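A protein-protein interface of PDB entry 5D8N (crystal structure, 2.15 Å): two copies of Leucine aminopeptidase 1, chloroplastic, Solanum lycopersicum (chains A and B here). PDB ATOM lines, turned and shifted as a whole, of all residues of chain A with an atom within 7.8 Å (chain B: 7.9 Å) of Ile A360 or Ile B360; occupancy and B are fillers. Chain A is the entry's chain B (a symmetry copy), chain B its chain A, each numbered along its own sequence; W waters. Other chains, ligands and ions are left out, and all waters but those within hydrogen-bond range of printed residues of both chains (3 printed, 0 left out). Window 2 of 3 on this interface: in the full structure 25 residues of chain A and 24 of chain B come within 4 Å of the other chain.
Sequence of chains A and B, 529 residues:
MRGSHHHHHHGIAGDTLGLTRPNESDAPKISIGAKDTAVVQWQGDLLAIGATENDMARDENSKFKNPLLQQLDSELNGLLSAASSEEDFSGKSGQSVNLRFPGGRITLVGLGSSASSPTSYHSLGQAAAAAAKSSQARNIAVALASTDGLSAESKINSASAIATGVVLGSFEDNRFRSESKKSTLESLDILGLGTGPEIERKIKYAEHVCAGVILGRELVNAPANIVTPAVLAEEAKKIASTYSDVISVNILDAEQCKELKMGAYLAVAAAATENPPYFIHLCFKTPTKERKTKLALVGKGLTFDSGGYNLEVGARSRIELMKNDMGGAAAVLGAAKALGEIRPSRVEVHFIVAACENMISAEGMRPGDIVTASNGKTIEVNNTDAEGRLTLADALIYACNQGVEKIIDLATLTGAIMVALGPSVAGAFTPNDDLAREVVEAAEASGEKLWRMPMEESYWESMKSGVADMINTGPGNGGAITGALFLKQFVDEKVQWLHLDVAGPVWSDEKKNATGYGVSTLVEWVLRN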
ATOM      1  N   VAL A 268      31.398  -9.754  10.290  1.00  0.00           N
ATOM      2  CA  VAL A 268      30.287  -8.990  10.849  1.00  0.00           C
ATOM      3  C   VAL A 268      30.486  -7.504  10.587  1.00  0.00           C
ATOM      4  O   VAL A 268      29.548  -6.781  10.237  1.00  0.00           O
ATOM      5  CB  VAL A 268      30.201  -9.182  12.367  1.00  0.00           C
ATOM      6  CG1 VAL A 268      29.145  -8.258  12.989  1.00  0.00           C
ATOM      7  CG2 VAL A 268      29.877 -10.625  12.693  1.00  0.00           C
ATOM      8  N   ALA A 270      32.044  -6.130   8.064  1.00  0.00           N
ATOM      9  CA  ALA A 270      32.272  -5.810   6.646  1.00  0.00           C
ATOM     10  C   ALA A 270      31.233  -4.859   6.057  1.00  0.00           C
ATOM     11  O   ALA A 270      31.590  -3.985   5.250  1.00  0.00           O
ATOM     12  CB  ALA A 270      32.314  -7.092   5.820  1.00  0.00           C
ATOM     13  N   ALA A 271      29.967  -4.986   6.459  1.00  0.00           N
ATOM     14  CA  ALA A 271      28.939  -4.094   5.923  1.00  0.00           C
ATOM     15  C   ALA A 271      29.188  -2.616   6.226  1.00  0.00           C
ATOM     16  O   ALA A 271      28.968  -1.745   5.381  1.00  0.00           O
ATOM     17  CB  ALA A 271      27.561  -4.465   6.425  1.00  0.00           C
ATOM     18  N   ALA A 272      29.646  -2.351   7.444  1.00  0.00           N
ATOM     19  CA  ALA A 272      29.706  -1.000   7.979  1.00  0.00           C
ATOM     20  C   ALA A 272      30.975  -0.307   7.490  1.00  0.00           C
ATOM     21  O   ALA A 272      31.912  -0.078   8.257  1.00  0.00           O
ATOM     22  CB  ALA A 272      29.689  -1.041   9.494  1.00  0.00           C
ATOM     23  N   THR A 273      30.946   0.117   6.230  1.00  0.00           N
ATOM     24  CA  THR A 273      32.109   0.759   5.622  1.00  0.00           C
ATOM     25  C   THR A 273      32.293   2.203   6.103  1.00  0.00           C
ATOM     26  O   THR A 273      33.391   2.737   6.026  1.00  0.00           O
ATOM     27  CB  THR A 273      31.979   0.802   4.090  1.00  0.00           C
ATOM     28  OG1 THR A 273      30.780   1.504   3.738  1.00  0.00           O
ATOM     29  CG2 THR A 273      31.972  -0.601   3.516  1.00  0.00           C
ATOM     30  N   PHE A 304      26.088  -0.736  17.241  1.00  0.00           N
ATOM     31  CA  PHE A 304      24.726  -0.964  16.794  1.00  0.00           C
ATOM     32  C   PHE A 304      24.576  -2.391  16.230  1.00  0.00           C
ATOM     33  O   PHE A 304      25.396  -2.853  15.433  1.00  0.00           O
ATOM     34  CB  PHE A 304      24.339   0.028  15.696  1.00  0.00           C
ATOM     35  CG  PHE A 304      22.964  -0.224  15.139  1.00  0.00           C
ATOM     36  CD1 PHE A 304      21.844   0.020  15.903  1.00  0.00           C
ATOM     37  CD2 PHE A 304      22.807  -0.899  13.936  1.00  0.00           C
ATOM     38  CE1 PHE A 304      20.580  -0.247  15.395  1.00  0.00           C
ATOM     39  CE2 PHE A 304      21.553  -1.108  13.393  1.00  0.00           C
ATOM     40  CZ  PHE A 304      20.436  -0.820  14.147  1.00  0.00           C
ATOM     41  N   SER A 306      22.021  -4.570  13.887  1.00  0.00           N
ATOM     42  CA  SER A 306      20.933  -4.674  12.899  1.00  0.00           C
ATOM     43  C   SER A 306      19.883  -5.721  13.272  1.00  0.00           C
ATOM     44  O   SER A 306      18.740  -5.594  12.843  1.00  0.00           O
ATOM     45  CB  SER A 306      21.484  -5.051  11.507  1.00  0.00           C
ATOM     46  OG  SER A 306      21.619  -3.942  10.630  1.00  0.00           O
ATOM     47  N   GLY A 307      20.289  -6.791  13.958  1.00  0.00           N
ATOM     48  CA  GLY A 307      19.360  -7.689  14.651  1.00  0.00           C
ATOM     49  C   GLY A 307      19.030  -7.184  16.046  1.00  0.00           C
ATOM     50  O   GLY A 307      17.863  -6.983  16.384  1.00  0.00           O
ATOM     51  N   GLU A 357      30.017  -1.989  14.101  1.00  0.00           N
ATOM     52  CA  GLU A 357      28.568  -1.925  13.986  1.00  0.00           C
ATOM     53  C   GLU A 357      28.111  -2.907  12.933  1.00  0.00           C
ATOM     54  O   GLU A 357      28.846  -3.204  11.999  1.00  0.00           O
ATOM     55  CB  GLU A 357      28.063  -0.482  13.766  1.00  0.00           C
ATOM     56  CG  GLU A 357      28.536   0.209  12.513  1.00  0.00           C
ATOM     57  CD  GLU A 357      27.845   1.545  12.238  1.00  0.00           C
ATOM     58  OE1 GLU A 357      27.122   2.097  13.107  1.00  0.00           O
ATOM     59  OE2 GLU A 357      28.029   2.020  11.094  1.00  0.00           O
ATOM     60  N   ASN A 358      26.952  -3.500  13.172  1.00  0.00           N
ATOM     61  CA  ASN A 358      26.391  -4.488  12.299  1.00  0.00           C
ATOM     62  C   ASN A 358      25.350  -3.809  11.416  1.00  0.00           C
ATOM     63  O   ASN A 358      24.188  -3.675  11.784  1.00  0.00           O
ATOM     64  CB  ASN A 358      25.776  -5.637  13.107  1.00  0.00           C
ATOM     65  CG  ASN A 358      25.088  -6.663  12.223  1.00  0.00           C
ATOM     66  OD1 ASN A 358      25.310  -6.711  11.014  1.00  0.00           O
ATOM     67  ND2 ASN A 358      24.250  -7.494  12.820  1.00  0.00           N
ATOM     68  N   MET A 359      25.744  -3.546  10.178  1.00  0.00           N
ATOM     69  CA  MET A 359      24.911  -2.823   9.223  1.00  0.00           C
ATOM     70  C   MET A 359      24.541  -3.685   8.003  1.00  0.00           C
ATOM     71  O   MET A 359      24.892  -4.864   7.904  1.00  0.00           O
ATOM     72  CB  MET A 359      25.674  -1.579   8.751  1.00  0.00           C
ATOM     73  CG  MET A 359      26.030  -0.607   9.871  1.00  0.00           C
ATOM     74  SD  MET A 359      24.627   0.261  10.587  1.00  0.00           S
ATOM     75  CE  MET A 359      24.597   1.727   9.567  1.00  0.00           C
ATOM     76  N   ILE A 360      23.827  -3.054   7.072  1.00  0.00           N
ATOM     77  CA  ILE A 360      23.405  -3.674   5.834  1.00  0.00           C
ATOM     78  C   ILE A 360      23.899  -2.849   4.666  1.00  0.00           C
ATOM     79  O   ILE A 360      23.611  -1.639   4.560  1.00  0.00           O
ATOM     80  CB  ILE A 360      21.873  -3.735   5.779  1.00  0.00           C
ATOM     81  CG1 ILE A 360      21.365  -4.697   6.858  1.00  0.00           C
ATOM     82  CG2 ILE A 360      21.420  -4.203   4.421  1.00  0.00           C
ATOM     83  CD1 ILE A 360      19.892  -4.555   7.143  1.00  0.00           C
ATOM     84  N   SER A 361      24.636  -3.523   3.791  1.00  0.00           N
ATOM     85  CA  SER A 361      25.189  -2.867   2.610  1.00  0.00           C
ATOM     86  C   SER A 361      25.585  -3.951   1.633  1.00  0.00           C
ATOM     87  O   SER A 361      25.638  -5.144   1.998  1.00  0.00           O
ATOM     88  CB  SER A 361      26.401  -2.009   3.000  1.00  0.00           C
ATOM     89  OG  SER A 361      27.546  -2.813   3.286  1.00  0.00           O
ATOM     90  N   ALA A 362      26.045  -3.496   0.470  1.00  0.00           N
ATOM     91  CA  ALA A 362      26.566  -4.381  -0.558  1.00  0.00           C
ATOM     92  C   ALA A 362      27.831  -5.150  -0.135  1.00  0.00           C
ATOM     93  O   ALA A 362      28.116  -6.228  -0.674  1.00  0.00           O
ATOM     94  CB  ALA A 362      26.843  -3.581  -1.819  1.00  0.00           C
ATOM     95  N   GLU A 363      28.600  -4.558   0.787  1.00  0.00           N
ATOM     96  CA  GLU A 363      29.819  -5.151   1.305  1.00  0.00           C
ATOM     97  C   GLU A 363      29.567  -6.118   2.445  1.00  0.00           C
ATOM     98  O   GLU A 363      30.501  -6.710   2.982  1.00  0.00           O
ATOM     99  CB  GLU A 363      30.808  -4.059   1.743  1.00  0.00           C
ATOM    100  CG  GLU A 363      31.376  -3.217   0.602  1.00  0.00           C
ATOM    101  CD  GLU A 363      30.554  -1.971   0.292  1.00  0.00           C
ATOM    102  OE1 GLU A 363      29.498  -1.741   0.927  1.00  0.00           O
ATOM    103  OE2 GLU A 363      30.985  -1.182  -0.584  1.00  0.00           O
ATOM    104  N   GLY A 364      28.308  -6.327   2.802  1.00  0.00           N
ATOM    105  CA  GLY A 364      27.971  -7.059   4.021  1.00  0.00           C
ATOM    106  C   GLY A 364      27.960  -8.571   3.862  1.00  0.00           C
ATOM    107  O   GLY A 364      27.880  -9.121   2.746  1.00  0.00           O
ATOM    108  N   MET A 365      27.977  -9.243   5.007  1.00  0.00           N
ATOM    109  CA  MET A 365      27.807 -10.689   5.080  1.00  0.00           C
ATOM    110  C   MET A 365      26.354 -11.064   4.814  1.00  0.00           C
ATOM    111  O   MET A 365      25.465 -10.346   5.206  1.00  0.00           O
ATOM    112  CB  MET A 365      28.243 -11.165   6.460  1.00  0.00           C
ATOM    113  CG  MET A 365      28.000 -12.641   6.719  1.00  0.00           C
ATOM    114  SD  MET A 365      28.768 -13.226   8.237  1.00  0.00           S
ATOM    115  CE  MET A 365      28.012 -12.124   9.433  1.00  0.00           C
ATOM    116  N   THR A 384      21.441 -13.964  10.756  1.00  0.00           N
ATOM    117  CA  THR A 384      22.158 -12.686  10.857  1.00  0.00           C
ATOM    118  C   THR A 384      21.720 -11.790  12.015  1.00  0.00           C
ATOM    119  O   THR A 384      22.373 -10.797  12.311  1.00  0.00           O
ATOM    120  CB  THR A 384      22.070 -11.887   9.537  1.00  0.00           C
ATOM    121  OG1 THR A 384      20.699 -11.706   9.158  1.00  0.00           O
ATOM    122  CG2 THR A 384      22.832 -12.648   8.427  1.00  0.00           C
ATOM    123  N   VAL B 268      18.193  -5.909 -10.931  1.00  0.00           N
ATOM    124  CA  VAL B 268      18.348  -6.832  -9.808  1.00  0.00           C
ATOM    125  C   VAL B 268      19.772  -6.791  -9.317  1.00  0.00           C
ATOM    126  O   VAL B 268      20.025  -6.756  -8.125  1.00  0.00           O
ATOM    127  CB  VAL B 268      18.016  -8.284 -10.238  1.00  0.00           C
ATOM    128  CG1 VAL B 268      18.287  -9.247  -9.094  1.00  0.00           C
ATOM    129  CG2 VAL B 268      16.550  -8.386 -10.639  1.00  0.00           C
ATOM    130  N   ALA B 270      21.927  -4.325  -9.417  1.00  0.00           N
ATOM    131  CA  ALA B 270      22.450  -2.989  -9.153  1.00  0.00           C
ATOM    132  C   ALA B 270      22.903  -2.803  -7.704  1.00  0.00           C
ATOM    133  O   ALA B 270      23.885  -2.115  -7.437  1.00  0.00           O
ATOM    134  CB  ALA B 270      21.401  -1.937  -9.512  1.00  0.00           C
ATOM    135  N   ALA B 271      22.220  -3.437  -6.760  1.00  0.00           N
ATOM    136  CA  ALA B 271      22.583  -3.211  -5.350  1.00  0.00           C
ATOM    137  C   ALA B 271      23.994  -3.732  -5.064  1.00  0.00           C
ATOM    138  O   ALA B 271      24.728  -3.133  -4.264  1.00  0.00           O
ATOM    139  CB  ALA B 271      21.579  -3.883  -4.417  1.00  0.00           C
ATOM    140  N   ALA B 272      24.340  -4.861  -5.686  1.00  0.00           N
ATOM    141  CA  ALA B 272      25.513  -5.648  -5.319  1.00  0.00           C
ATOM    142  C   ALA B 272      26.759  -5.092  -5.990  1.00  0.00           C
ATOM    143  O   ALA B 272      27.293  -5.684  -6.937  1.00  0.00           O
ATOM    144  CB  ALA B 272      25.318  -7.098  -5.707  1.00  0.00           C
ATOM    145  N   THR B 273      27.247  -3.981  -5.453  1.00  0.00           N
ATOM    146  CA  THR B 273      28.384  -3.292  -6.063  1.00  0.00           C
ATOM    147  C   THR B 273      29.710  -4.003  -5.774  1.00  0.00           C
ATOM    148  O   THR B 273      30.693  -3.804  -6.482  1.00  0.00           O
ATOM    149  CB  THR B 273      28.479  -1.851  -5.544  1.00  0.00           C
ATOM    150  OG1 THR B 273      28.577  -1.870  -4.114  1.00  0.00           O
ATOM    151  CG2 THR B 273      27.241  -1.029  -5.982  1.00  0.00           C
ATOM    152  N   PHE B 304      23.202 -15.344  -4.471  1.00  0.00           N
ATOM    153  CA  PHE B 304      22.440 -15.129  -3.245  1.00  0.00           C
ATOM    154  C   PHE B 304      21.173 -14.341  -3.571  1.00  0.00           C
ATOM    155  O   PHE B 304      21.204 -13.341  -4.309  1.00  0.00           O
ATOM    156  CB  PHE B 304      23.273 -14.341  -2.218  1.00  0.00           C
ATOM    157  CG  PHE B 304      22.520 -13.993  -0.967  1.00  0.00           C
ATOM    158  CD1 PHE B 304      22.216 -14.957  -0.029  1.00  0.00           C
ATOM    159  CD2 PHE B 304      22.031 -12.712  -0.778  1.00  0.00           C
ATOM    160  CE1 PHE B 304      21.389 -14.672   1.042  1.00  0.00           C
ATOM    161  CE2 PHE B 304      21.213 -12.420   0.302  1.00  0.00           C
ATOM    162  CZ  PHE B 304      20.882 -13.404   1.212  1.00  0.00           C
ATOM    163  N   SER B 306      18.329 -12.165  -1.629  1.00  0.00           N
ATOM    164  CA  SER B 306      17.882 -11.376  -0.471  1.00  0.00           C
ATOM    165  C   SER B 306      16.445 -11.673  -0.042  1.00  0.00           C
ATOM    166  O   SER B 306      16.102 -11.482   1.130  1.00  0.00           O
ATOM    167  CB  SER B 306      17.954  -9.865  -0.773  1.00  0.00           C
ATOM    168  OG  SER B 306      19.069  -9.208  -0.188  1.00  0.00           O
ATOM    169  N   GLY B 307      15.586 -11.993  -1.005  1.00  0.00           N
ATOM    170  CA  GLY B 307      14.214 -12.388  -0.699  1.00  0.00           C
ATOM    171  C   GLY B 307      14.007 -13.835  -0.286  1.00  0.00           C
ATOM    172  O   GLY B 307      14.908 -14.479   0.245  1.00  0.00           O
ATOM    173  N   GLU B 357      24.165 -11.340  -7.567  1.00  0.00           N
ATOM    174  CA  GLU B 357      23.608 -11.498  -6.236  1.00  0.00           C
ATOM    175  C   GLU B 357      22.656 -10.357  -5.948  1.00  0.00           C
ATOM    176  O   GLU B 357      22.778  -9.273  -6.505  1.00  0.00           O
ATOM    177  CB  GLU B 357      24.681 -11.659  -5.152  1.00  0.00           C
ATOM    178  CG  GLU B 357      25.623 -10.496  -4.977  1.00  0.00           C
ATOM    179  CD  GLU B 357      26.568 -10.630  -3.805  1.00  0.00           C
ATOM    180  OE1 GLU B 357      26.590 -11.694  -3.129  1.00  0.00           O
ATOM    181  OE2 GLU B 357      27.122  -9.562  -3.437  1.00  0.00           O
ATOM    182  N   ASN B 358      21.561 -10.713  -5.287  1.00  0.00           N
ATOM    183  CA  ASN B 358      20.499  -9.769  -4.988  1.00  0.00           C
ATOM    184  C   ASN B 358      20.678  -9.222  -3.571  1.00  0.00           C
ATOM    185  O   ASN B 358      20.343  -9.898  -2.595  1.00  0.00           O
ATOM    186  CB  ASN B 358      19.132 -10.446  -5.147  1.00  0.00           C
ATOM    187  CG  ASN B 358      17.983  -9.513  -4.789  1.00  0.00           C
ATOM    188  OD1 ASN B 358      18.190  -8.316  -4.606  1.00  0.00           O
ATOM    189  ND2 ASN B 358      16.792 -10.077  -4.596  1.00  0.00           N
ATOM    190  N   MET B 359      21.254  -8.035  -3.478  1.00  0.00           N
ATOM    191  CA  MET B 359      21.639  -7.425  -2.219  1.00  0.00           C
ATOM    192  C   MET B 359      20.816  -6.158  -1.911  1.00  0.00           C
ATOM    193  O   MET B 359      19.907  -5.778  -2.650  1.00  0.00           O
ATOM    194  CB  MET B 359      23.124  -7.051  -2.266  1.00  0.00           C
ATOM    195  CG  MET B 359      24.062  -8.230  -2.443  1.00  0.00           C
ATOM    196  SD  MET B 359      24.152  -9.312  -1.002  1.00  0.00           S
ATOM    197  CE  MET B 359      25.529  -8.604  -0.117  1.00  0.00           C
ATOM    198  N   ILE B 360      21.151  -5.539  -0.783  1.00  0.00           N
ATOM    199  CA  ILE B 360      20.527  -4.305  -0.321  1.00  0.00           C
ATOM    200  C   ILE B 360      21.587  -3.230  -0.106  1.00  0.00           C
ATOM    201  O   ILE B 360      22.556  -3.429   0.645  1.00  0.00           O
ATOM    202  CB  ILE B 360      19.810  -4.565   1.016  1.00  0.00           C
ATOM    203  CG1 ILE B 360      18.638  -5.522   0.783  1.00  0.00           C
ATOM    204  CG2 ILE B 360      19.327  -3.255   1.600  1.00  0.00           C
ATOM    205  CD1 ILE B 360      18.091  -6.129   2.052  1.00  0.00           C
ATOM    206  N   SER B 361      21.394  -2.105  -0.790  1.00  0.00           N
ATOM    207  CA  SER B 361      22.340  -0.993  -0.728  1.00  0.00           C
ATOM    208  C   SER B 361      21.708   0.253  -1.322  1.00  0.00           C
ATOM    209  O   SER B 361      20.608   0.220  -1.882  1.00  0.00           O
ATOM    210  CB  SER B 361      23.604  -1.312  -1.531  1.00  0.00           C
ATOM    211  OG  SER B 361      23.355  -1.201  -2.925  1.00  0.00           O
ATOM    212  N   ALA B 362      22.417   1.363  -1.198  1.00  0.00           N
ATOM    213  CA  ALA B 362      21.921   2.637  -1.746  1.00  0.00           C
ATOM    214  C   ALA B 362      21.743   2.605  -3.276  1.00  0.00           C
ATOM    215  O   ALA B 362      20.980   3.412  -3.829  1.00  0.00           O
ATOM    216  CB  ALA B 362      22.854   3.775  -1.339  1.00  0.00           C
ATOM    217  N   GLU B 363      22.511   1.735  -3.937  1.00  0.00           N
ATOM    218  CA  GLU B 363      22.504   1.595  -5.390  1.00  0.00           C
ATOM    219  C   GLU B 363      21.431   0.606  -5.850  1.00  0.00           C
ATOM    220  O   GLU B 363      21.232   0.419  -7.051  1.00  0.00           O
ATOM    221  CB  GLU B 363      23.875   1.137  -5.904  1.00  0.00           C
ATOM    222  CG  GLU B 363      24.984   2.176  -5.770  1.00  0.00           C
ATOM    223  CD  GLU B 363      25.752   2.085  -4.454  1.00  0.00           C
ATOM    224  OE1 GLU B 363      25.412   1.214  -3.602  1.00  0.00           O
ATOM    225  OE2 GLU B 363      26.729   2.870  -4.294  1.00  0.00           O
ATOM    226  N   GLY B 364      20.643   0.093  -4.912  1.00  0.00           N
ATOM    227  CA  GLY B 364      19.703  -0.982  -5.218  1.00  0.00           C
ATOM    228  C   GLY B 364      18.369  -0.569  -5.806  1.00  0.00           C
ATOM    229  O   GLY B 364      17.933   0.575  -5.649  1.00  0.00           O
ATOM    230  N   MET B 365      17.678  -1.550  -6.388  1.00  0.00           N
ATOM    231  CA  MET B 365      16.289  -1.412  -6.824  1.00  0.00           C
ATOM    232  C   MET B 365      15.351  -1.365  -5.616  1.00  0.00           C
ATOM    233  O   MET B 365      15.584  -2.038  -4.632  1.00  0.00           O
ATOM    234  CB  MET B 365      15.922  -2.580  -7.740  1.00  0.00           C
ATOM    235  CG  MET B 365      14.481  -2.603  -8.193  1.00  0.00           C
ATOM    236  SD  MET B 365      14.171  -3.817  -9.495  1.00  0.00           S
ATOM    237  CE  MET B 365      14.697  -5.330  -8.728  1.00  0.00           C
ATOM    238  N   THR B 384      10.035  -7.485  -4.081  1.00  0.00           N
ATOM    239  CA  THR B 384      11.475  -7.674  -4.202  1.00  0.00           C
ATOM    240  C   THR B 384      12.000  -9.043  -3.758  1.00  0.00           C
ATOM    241  O   THR B 384      13.163  -9.368  -3.991  1.00  0.00           O
ATOM    242  CB  THR B 384      12.260  -6.586  -3.443  1.00  0.00           C
ATOM    243  OG1 THR B 384      11.827  -6.556  -2.082  1.00  0.00           O
ATOM    244  CG2 THR B 384      12.043  -5.215  -4.113  1.00  0.00           C
HETATM  245  O   HOH W   1      22.931  -6.324   1.505  1.00  0.00           O
HETATM  246  O   HOH W   2      31.001  -2.014  -3.225  1.00  0.00           O
HETATM  247  O   HOH W   3      27.802  -6.916  -3.340  1.00  0.00           O
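Ile B360 touches its own counterpart, Ile A360.
Ala A362 touches Thr B273, but with the chains exchanged Thr A273 does not touch Ala B362 (9.7 Å).
Ala A362 touches Met B359, but with the chains exchanged Met A359 does not touch Ala B362 (10.7 Å).
Ala A362 touches Ser B361, but with the chains exchanged Ser A361 does not touch Ala B362 (6.3 Å).
The backbone NH of Glu B363 sits close to the side-chain hydroxyl of Ser B361, at 3.2 Å.
The side-chain hydroxyl of Ser A361 sits at hydrogen-bond distance from the backbone carbonyl oxygen of Ala A271 (2.7 Å).
O of Ala B271 sits at hydrogen-bond distance from OG of Ser B361.
The side-chain hydroxyl (OG) of Ser A361 lies close to the backbone NH (N) of Glu A363 (3.2 Å).
Water W2 lies within hydrogen-bond range of the side-chain hydroxyl of Thr B273 (2.6 Å) and the side-chain carboxylate of Glu A363 (2.8 Å).
Water W3 lies within hydrogen-bond range of the side-chain carboxylate (OE2) of Glu B357 and the backbone carbonyl oxygen (O) of Ala A362.
Water W1 bridges the backbone carbonyl oxygen (O) of Ser A361 and the backbone NH (N) of Ile B360.
The backbone carbonyl oxygen (O) of Ile B360 sits at hydrogen-bond distance from the backbone NH (N) of Ala A362, at 3.5 Å.
CG2 of Ile A360 touches CG2 of Ile B360, 3.6 Å away.
Ser A361 touches Ile B360.
Ala A362 touches Ala B271.
Ala A362 touches Thr B273.
CE of Met B359 touches O of Ala A362 (3.6 Å).
N of Ala A362 touches CB of Ser B361 (3.8 Å).
Met B359 touches Gly A364.
Along chain A the printed residues that touch a printed residue of chain B span positions 360 to 364.
Of chain B, only Ile B360 comes within 4 Å of Ile A360.
Of the printed residues of chain A, Met B359 touches Ala A362 and Gly A364.
Of the printed residues of chain B, Gly A364 touches Met B359.
Of the printed residues of chain A, Thr B273 touches Ala A362 (3.3 Å).
Printed residues of chain A within 4 Å of Ala B271: Ala A362 (3.3 Å).
The nearest residue of chain A that does not touch Ile B360 is Glu A363 (6.2 Å).
The nearest printed residue of chain B that does not touch Ser A361 is Met B359 (4.1 Å).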
